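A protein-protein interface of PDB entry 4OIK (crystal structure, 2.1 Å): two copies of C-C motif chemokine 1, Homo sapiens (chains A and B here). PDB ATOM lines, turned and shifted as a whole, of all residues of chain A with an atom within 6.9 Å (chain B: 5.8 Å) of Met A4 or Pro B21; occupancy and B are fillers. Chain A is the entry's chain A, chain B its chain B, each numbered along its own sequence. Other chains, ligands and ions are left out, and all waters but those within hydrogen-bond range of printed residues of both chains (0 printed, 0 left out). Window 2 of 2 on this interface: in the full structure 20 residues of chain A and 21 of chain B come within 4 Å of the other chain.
The backbone NH (N) of Val A6 lies close to the backbone carbonyl oxygen (O) of Glu B49, at 3.5 Å.
The side-chain hydroxyl (OG) of Ser A3 lies within hydrogen-bond range of the side-chain amide nitrogen (NE2) of Gln A5 (2.9 Å).
The backbone carbonyl oxygen (O) of Ile B20 is in hydrogen-bond range of a ring nitrogen (NE2) of His B62 (2.7 Å).
Met A4 touches Ile B20 (SD to CG2, 3.9 Å).
CD of Pro B21 touches SD of Met A4 (3.6 Å).
Glu B49 touches Gln A5.
N of Ala B16 touches CG1 of Val A6 (3.6 Å).
Val A6 touches Ala B50.
Printed residues of chain B within 4 Å of Met A4: Ile B20 (3.9 Å) and Pro B21 (3.6 Å).
Printed residues of chain B within 4 Å of Gln A5: Glu B49.
Printed residues of chain B within 4 Å of Val A6: Ala B16 (3.6 Å), Glu B49 (3.5 Å) and Ala B50 (3.5 Å).
Of the printed residues of chain A, Pro B21 touches Met A4 (3.6 Å).
Of the printed residues of chain A, Glu B49 touches Gln A5 (3.1 Å) and Val A6 (3.5 Å).
Of the printed residues of chain A, Ala B50 touches Val A6 (3.5 Å).
The nearest printed residue of chain B that does not touch Met A4 is Ala B50 (4.02 Å).
Of the 6 printed residues of chain A, 3 touch a printed residue of chain B.
Hydrophobic or aromatic side chains of chain A that line the printed part of chain B: Met A4 and Val A6.
Of the 12 printed residues of chain B, 5 touch a printed residue of chain A.
Hydrophobic or aromatic side chains of chain B that line the printed part of chain A: Ala B16, Ile B20, Pro B21 and Ala B50.
Among the printed residues, 6 pairs touch across the chains.
Among the printed residues, no Asp or Glu carboxylate lies within 4 Å of a Lys or Arg side-chain nitrogen of the other chain.
No position is printed for both chains.
Of the 6 pairs that touch across the chains among the printed residues, none has its exchanged pair printed and touching as well.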
ATOM      1  N   SER A   1      14.752   5.037 -15.968  1.00  0.00           N
ATOM      2  CA  SER A   1      13.873   4.048 -16.584  1.00  0.00           C
ATOM      3  C   SER A   1      12.437   4.165 -16.039  1.00  0.00           C
ATOM      4  O   SER A   1      12.121   3.595 -14.987  1.00  0.00           O
ATOM      5  CB  SER A   1      14.433   2.638 -16.395  1.00  0.00           C
ATOM      6  OG  SER A   1      13.565   1.648 -16.926  1.00  0.00           O
ATOM      7  N   LYS A   2      11.571   4.918 -16.759  1.00  0.00           N
ATOM      8  CA  LYS A   2      10.174   5.138 -16.378  1.00  0.00           C
ATOM      9  C   LYS A   2       9.329   3.897 -16.656  1.00  0.00           C
ATOM     10  O   LYS A   2       9.196   3.483 -17.815  1.00  0.00           O
ATOM     11  CB  LYS A   2       9.575   6.367 -17.099  1.00  0.00           C
ATOM     12  CG  LYS A   2      10.279   7.704 -16.854  1.00  0.00           C
ATOM     13  CD  LYS A   2       9.742   8.501 -15.646  1.00  0.00           C
ATOM     14  CE  LYS A   2       8.569   9.399 -15.982  1.00  0.00           C
ATOM     15  NZ  LYS A   2       8.997  10.740 -16.468  1.00  0.00           N
ATOM     16  N   SER A   3       8.780   3.294 -15.580  1.00  0.00           N
ATOM     17  CA  SER A   3       7.942   2.099 -15.662  1.00  0.00           C
ATOM     18  C   SER A   3       6.699   2.082 -14.757  1.00  0.00           C
ATOM     19  O   SER A   3       6.665   1.417 -13.716  1.00  0.00           O
ATOM     20  CB  SER A   3       8.767   0.819 -15.550  1.00  0.00           C
ATOM     21  OG  SER A   3       9.159   0.353 -16.831  1.00  0.00           O
ATOM     22  N   MET A   4       5.670   2.821 -15.195  1.00  0.00           N
ATOM     23  CA  MET A   4       4.320   2.875 -14.625  1.00  0.00           C
ATOM     24  C   MET A   4       3.519   1.964 -15.557  1.00  0.00           C
ATOM     25  O   MET A   4       2.302   1.806 -15.414  1.00  0.00           O
ATOM     26  CB  MET A   4       3.745   4.294 -14.745  1.00  0.00           C
ATOM     27  CG  MET A   4       4.270   5.269 -13.748  1.00  0.00           C
ATOM     28  SD  MET A   4       3.430   6.844 -14.014  1.00  0.00           S
ATOM     29  CE  MET A   4       4.495   7.931 -13.063  1.00  0.00           C
ATOM     30  N   GLN A   5       4.248   1.387 -16.531  1.00  0.00           N
ATOM     31  CA  GLN A   5       3.820   0.550 -17.640  1.00  0.00           C
ATOM     32  C   GLN A   5       3.386  -0.896 -17.370  1.00  0.00           C
ATOM     33  O   GLN A   5       4.039  -1.662 -16.654  1.00  0.00           O
ATOM     34  CB  GLN A   5       4.855   0.608 -18.782  1.00  0.00           C
ATOM     35  CG  GLN A   5       6.242   0.051 -18.433  1.00  0.00           C
ATOM     36  CD  GLN A   5       7.048  -0.393 -19.634  1.00  0.00           C
ATOM     37  OE1 GLN A   5       6.538  -0.583 -20.756  1.00  0.00           O
ATOM     38  NE2 GLN A   5       8.345  -0.564 -19.417  1.00  0.00           N
ATOM     39  N   VAL A   6       2.302  -1.265 -18.049  1.00  0.00           N
ATOM     40  CA  VAL A   6       1.666  -2.583 -18.084  1.00  0.00           C
ATOM     41  C   VAL A   6       1.261  -2.718 -19.575  1.00  0.00           C
ATOM     42  O   VAL A   6       0.161  -2.352 -20.001  1.00  0.00           O
ATOM     43  CB  VAL A   6       0.559  -2.744 -17.001  1.00  0.00           C
ATOM     44  CG1 VAL A   6      -0.226  -1.457 -16.772  1.00  0.00           C
ATOM     45  CG2 VAL A   6      -0.346  -3.926 -17.266  1.00  0.00           C
ATOM     46  N   ALA B  16      -3.337  -1.677 -15.055  1.00  0.00           N
ATOM     47  CA  ALA B  16      -2.697  -0.808 -14.090  1.00  0.00           C
ATOM     48  C   ALA B  16      -3.496  -0.806 -12.804  1.00  0.00           C
ATOM     49  O   ALA B  16      -4.663  -0.425 -12.805  1.00  0.00           O
ATOM     50  CB  ALA B  16      -2.588   0.615 -14.645  1.00  0.00           C
ATOM     51  N   GLU B  19      -2.972   4.211  -9.931  1.00  0.00           N
ATOM     52  CA  GLU B  19      -3.378   5.329 -10.769  1.00  0.00           C
ATOM     53  C   GLU B  19      -2.125   5.992 -11.360  1.00  0.00           C
ATOM     54  O   GLU B  19      -1.167   6.291 -10.633  1.00  0.00           O
ATOM     55  CB  GLU B  19      -4.193   6.354  -9.954  1.00  0.00           C
ATOM     56  CG  GLU B  19      -4.683   7.519 -10.805  1.00  0.00           C
ATOM     57  CD  GLU B  19      -5.181   8.748 -10.081  1.00  0.00           C
ATOM     58  OE1 GLU B  19      -6.412   8.854  -9.881  1.00  0.00           O
ATOM     59  OE2 GLU B  19      -4.352   9.635  -9.775  1.00  0.00           O
ATOM     60  N   ILE B  20      -2.134   6.173 -12.680  1.00  0.00           N
ATOM     61  CA  ILE B  20      -1.074   6.836 -13.444  1.00  0.00           C
ATOM     62  C   ILE B  20      -1.449   8.324 -13.468  1.00  0.00           C
ATOM     63  O   ILE B  20      -2.605   8.628 -13.781  1.00  0.00           O
ATOM     64  CB  ILE B  20      -1.004   6.261 -14.896  1.00  0.00           C
ATOM     65  CG1 ILE B  20      -0.682   4.768 -14.907  1.00  0.00           C
ATOM     66  CG2 ILE B  20      -0.011   7.061 -15.775  1.00  0.00           C
ATOM     67  CD1 ILE B  20      -1.391   4.035 -15.967  1.00  0.00           C
ATOM     68  N   PRO B  21      -0.520   9.265 -13.163  1.00  0.00           N
ATOM     69  CA  PRO B  21      -0.881  10.694 -13.216  1.00  0.00           C
ATOM     70  C   PRO B  21      -1.198  11.172 -14.634  1.00  0.00           C
ATOM     71  O   PRO B  21      -0.475  10.840 -15.574  1.00  0.00           O
ATOM     72  CB  PRO B  21       0.371  11.396 -12.686  1.00  0.00           C
ATOM     73  CG  PRO B  21       1.185  10.317 -12.021  1.00  0.00           C
ATOM     74  CD  PRO B  21       0.892   9.089 -12.771  1.00  0.00           C
ATOM     75  N   LEU B  22      -2.269  11.968 -14.778  1.00  0.00           N
ATOM     76  CA  LEU B  22      -2.730  12.547 -16.043  1.00  0.00           C
ATOM     77  C   LEU B  22      -1.587  13.211 -16.824  1.00  0.00           C
ATOM     78  O   LEU B  22      -1.456  12.977 -18.025  1.00  0.00           O
ATOM     79  CB  LEU B  22      -3.871  13.553 -15.762  1.00  0.00           C
ATOM     80  CG  LEU B  22      -4.712  14.039 -16.948  1.00  0.00           C
ATOM     81  CD1 LEU B  22      -5.330  12.872 -17.741  1.00  0.00           C
ATOM     82  CD2 LEU B  22      -5.794  14.991 -16.484  1.00  0.00           C
ATOM     83  N   ARG B  23      -0.728  13.982 -16.121  1.00  0.00           N
ATOM     84  CA  ARG B  23       0.452  14.696 -16.664  1.00  0.00           C
ATOM     85  C   ARG B  23       1.449  13.770 -17.377  1.00  0.00           C
ATOM     86  O   ARG B  23       2.164  14.213 -18.273  1.00  0.00           O
ATOM     87  CB  ARG B  23       1.184  15.478 -15.550  1.00  0.00           C
ATOM     88  CG  ARG B  23       1.550  14.609 -14.330  1.00  0.00           C
ATOM     89  CD  ARG B  23       2.540  15.262 -13.368  1.00  0.00           C
ATOM     90  NE  ARG B  23       2.583  14.570 -12.072  1.00  0.00           N
ATOM     91  CZ  ARG B  23       3.242  13.435 -11.838  1.00  0.00           C
ATOM     92  NH1 ARG B  23       3.217  12.883 -10.633  1.00  0.00           N
ATOM     93  NH2 ARG B  23       3.915  12.833 -12.815  1.00  0.00           N
ATOM     94  N   ALA B  24       1.484  12.490 -16.968  1.00  0.00           N
ATOM     95  CA  ALA B  24       2.376  11.458 -17.492  1.00  0.00           C
ATOM     96  C   ALA B  24       1.850  10.807 -18.781  1.00  0.00           C
ATOM     97  O   ALA B  24       2.573  10.022 -19.397  1.00  0.00           O
ATOM     98  CB  ALA B  24       2.596  10.388 -16.418  1.00  0.00           C
ATOM     99  N   ILE B  25       0.601  11.150 -19.188  1.00  0.00           N
ATOM    100  CA  ILE B  25      -0.118  10.564 -20.327  1.00  0.00           C
ATOM    101  C   ILE B  25      -0.296  11.571 -21.456  1.00  0.00           C
ATOM    102  O   ILE B  25      -0.718  12.696 -21.204  1.00  0.00           O
ATOM    103  CB  ILE B  25      -1.499  10.018 -19.864  1.00  0.00           C
ATOM    104  CG1 ILE B  25      -1.392   9.141 -18.578  1.00  0.00           C
ATOM    105  CG2 ILE B  25      -2.203   9.258 -21.000  1.00  0.00           C
ATOM    106  CD1 ILE B  25      -2.778   8.736 -17.854  1.00  0.00           C
ATOM    107  N   LEU B  44       2.081   6.638 -22.765  1.00  0.00           N
ATOM    108  CA  LEU B  44       2.908   7.404 -21.829  1.00  0.00           C
ATOM    109  C   LEU B  44       4.078   8.037 -22.591  1.00  0.00           C
ATOM    110  O   LEU B  44       4.165   7.901 -23.808  1.00  0.00           O
ATOM    111  CB  LEU B  44       3.429   6.501 -20.689  1.00  0.00           C
ATOM    112  CG  LEU B  44       2.417   5.594 -19.957  1.00  0.00           C
ATOM    113  CD1 LEU B  44       3.139   4.647 -19.014  1.00  0.00           C
ATOM    114  CD2 LEU B  44       1.410   6.413 -19.174  1.00  0.00           C
ATOM    115  N   GLU B  49       3.649   2.558 -22.609  1.00  0.00           N
ATOM    116  CA  GLU B  49       2.194   2.413 -22.631  1.00  0.00           C
ATOM    117  C   GLU B  49       1.681   1.686 -21.393  1.00  0.00           C
ATOM    118  O   GLU B  49       2.451   1.015 -20.700  1.00  0.00           O
ATOM    119  CB  GLU B  49       1.747   1.676 -23.896  1.00  0.00           C
ATOM    120  CG  GLU B  49       1.077   2.585 -24.914  1.00  0.00           C
ATOM    121  CD  GLU B  49       1.680   2.636 -26.301  1.00  0.00           C
ATOM    122  OE1 GLU B  49       2.927   2.618 -26.413  1.00  0.00           O
ATOM    123  OE2 GLU B  49       0.902   2.782 -27.273  1.00  0.00           O
ATOM    124  N   ALA B  50       0.391   1.839 -21.088  1.00  0.00           N
ATOM    125  CA  ALA B  50      -0.184   1.130 -19.952  1.00  0.00           C
ATOM    126  C   ALA B  50      -1.633   0.780 -20.179  1.00  0.00           C
ATOM    127  O   ALA B  50      -2.425   1.637 -20.547  1.00  0.00           O
ATOM    128  CB  ALA B  50      -0.037   1.948 -18.679  1.00  0.00           C
ATOM    129  N   HIS B  62      -9.648  10.137 -16.348  1.00  0.00           N
ATOM    130  CA  HIS B  62      -8.492  10.441 -17.186  1.00  0.00           C
ATOM    131  C   HIS B  62      -8.887  10.400 -18.643  1.00  0.00           C
ATOM    132  O   HIS B  62      -8.590  11.355 -19.354  1.00  0.00           O
ATOM    133  CB  HIS B  62      -7.345   9.450 -16.937  1.00  0.00           C
ATOM    134  CG  HIS B  62      -6.561   9.695 -15.686  1.00  0.00           C
ATOM    135  ND1 HIS B  62      -6.917  10.681 -14.783  1.00  0.00           N
ATOM    136  CD2 HIS B  62      -5.454   9.067 -15.231  1.00  0.00           C
ATOM    137  CE1 HIS B  62      -6.028  10.615 -13.806  1.00  0.00           C
ATOM    138  NE2 HIS B  62      -5.136   9.647 -14.025  1.00  0.00           N
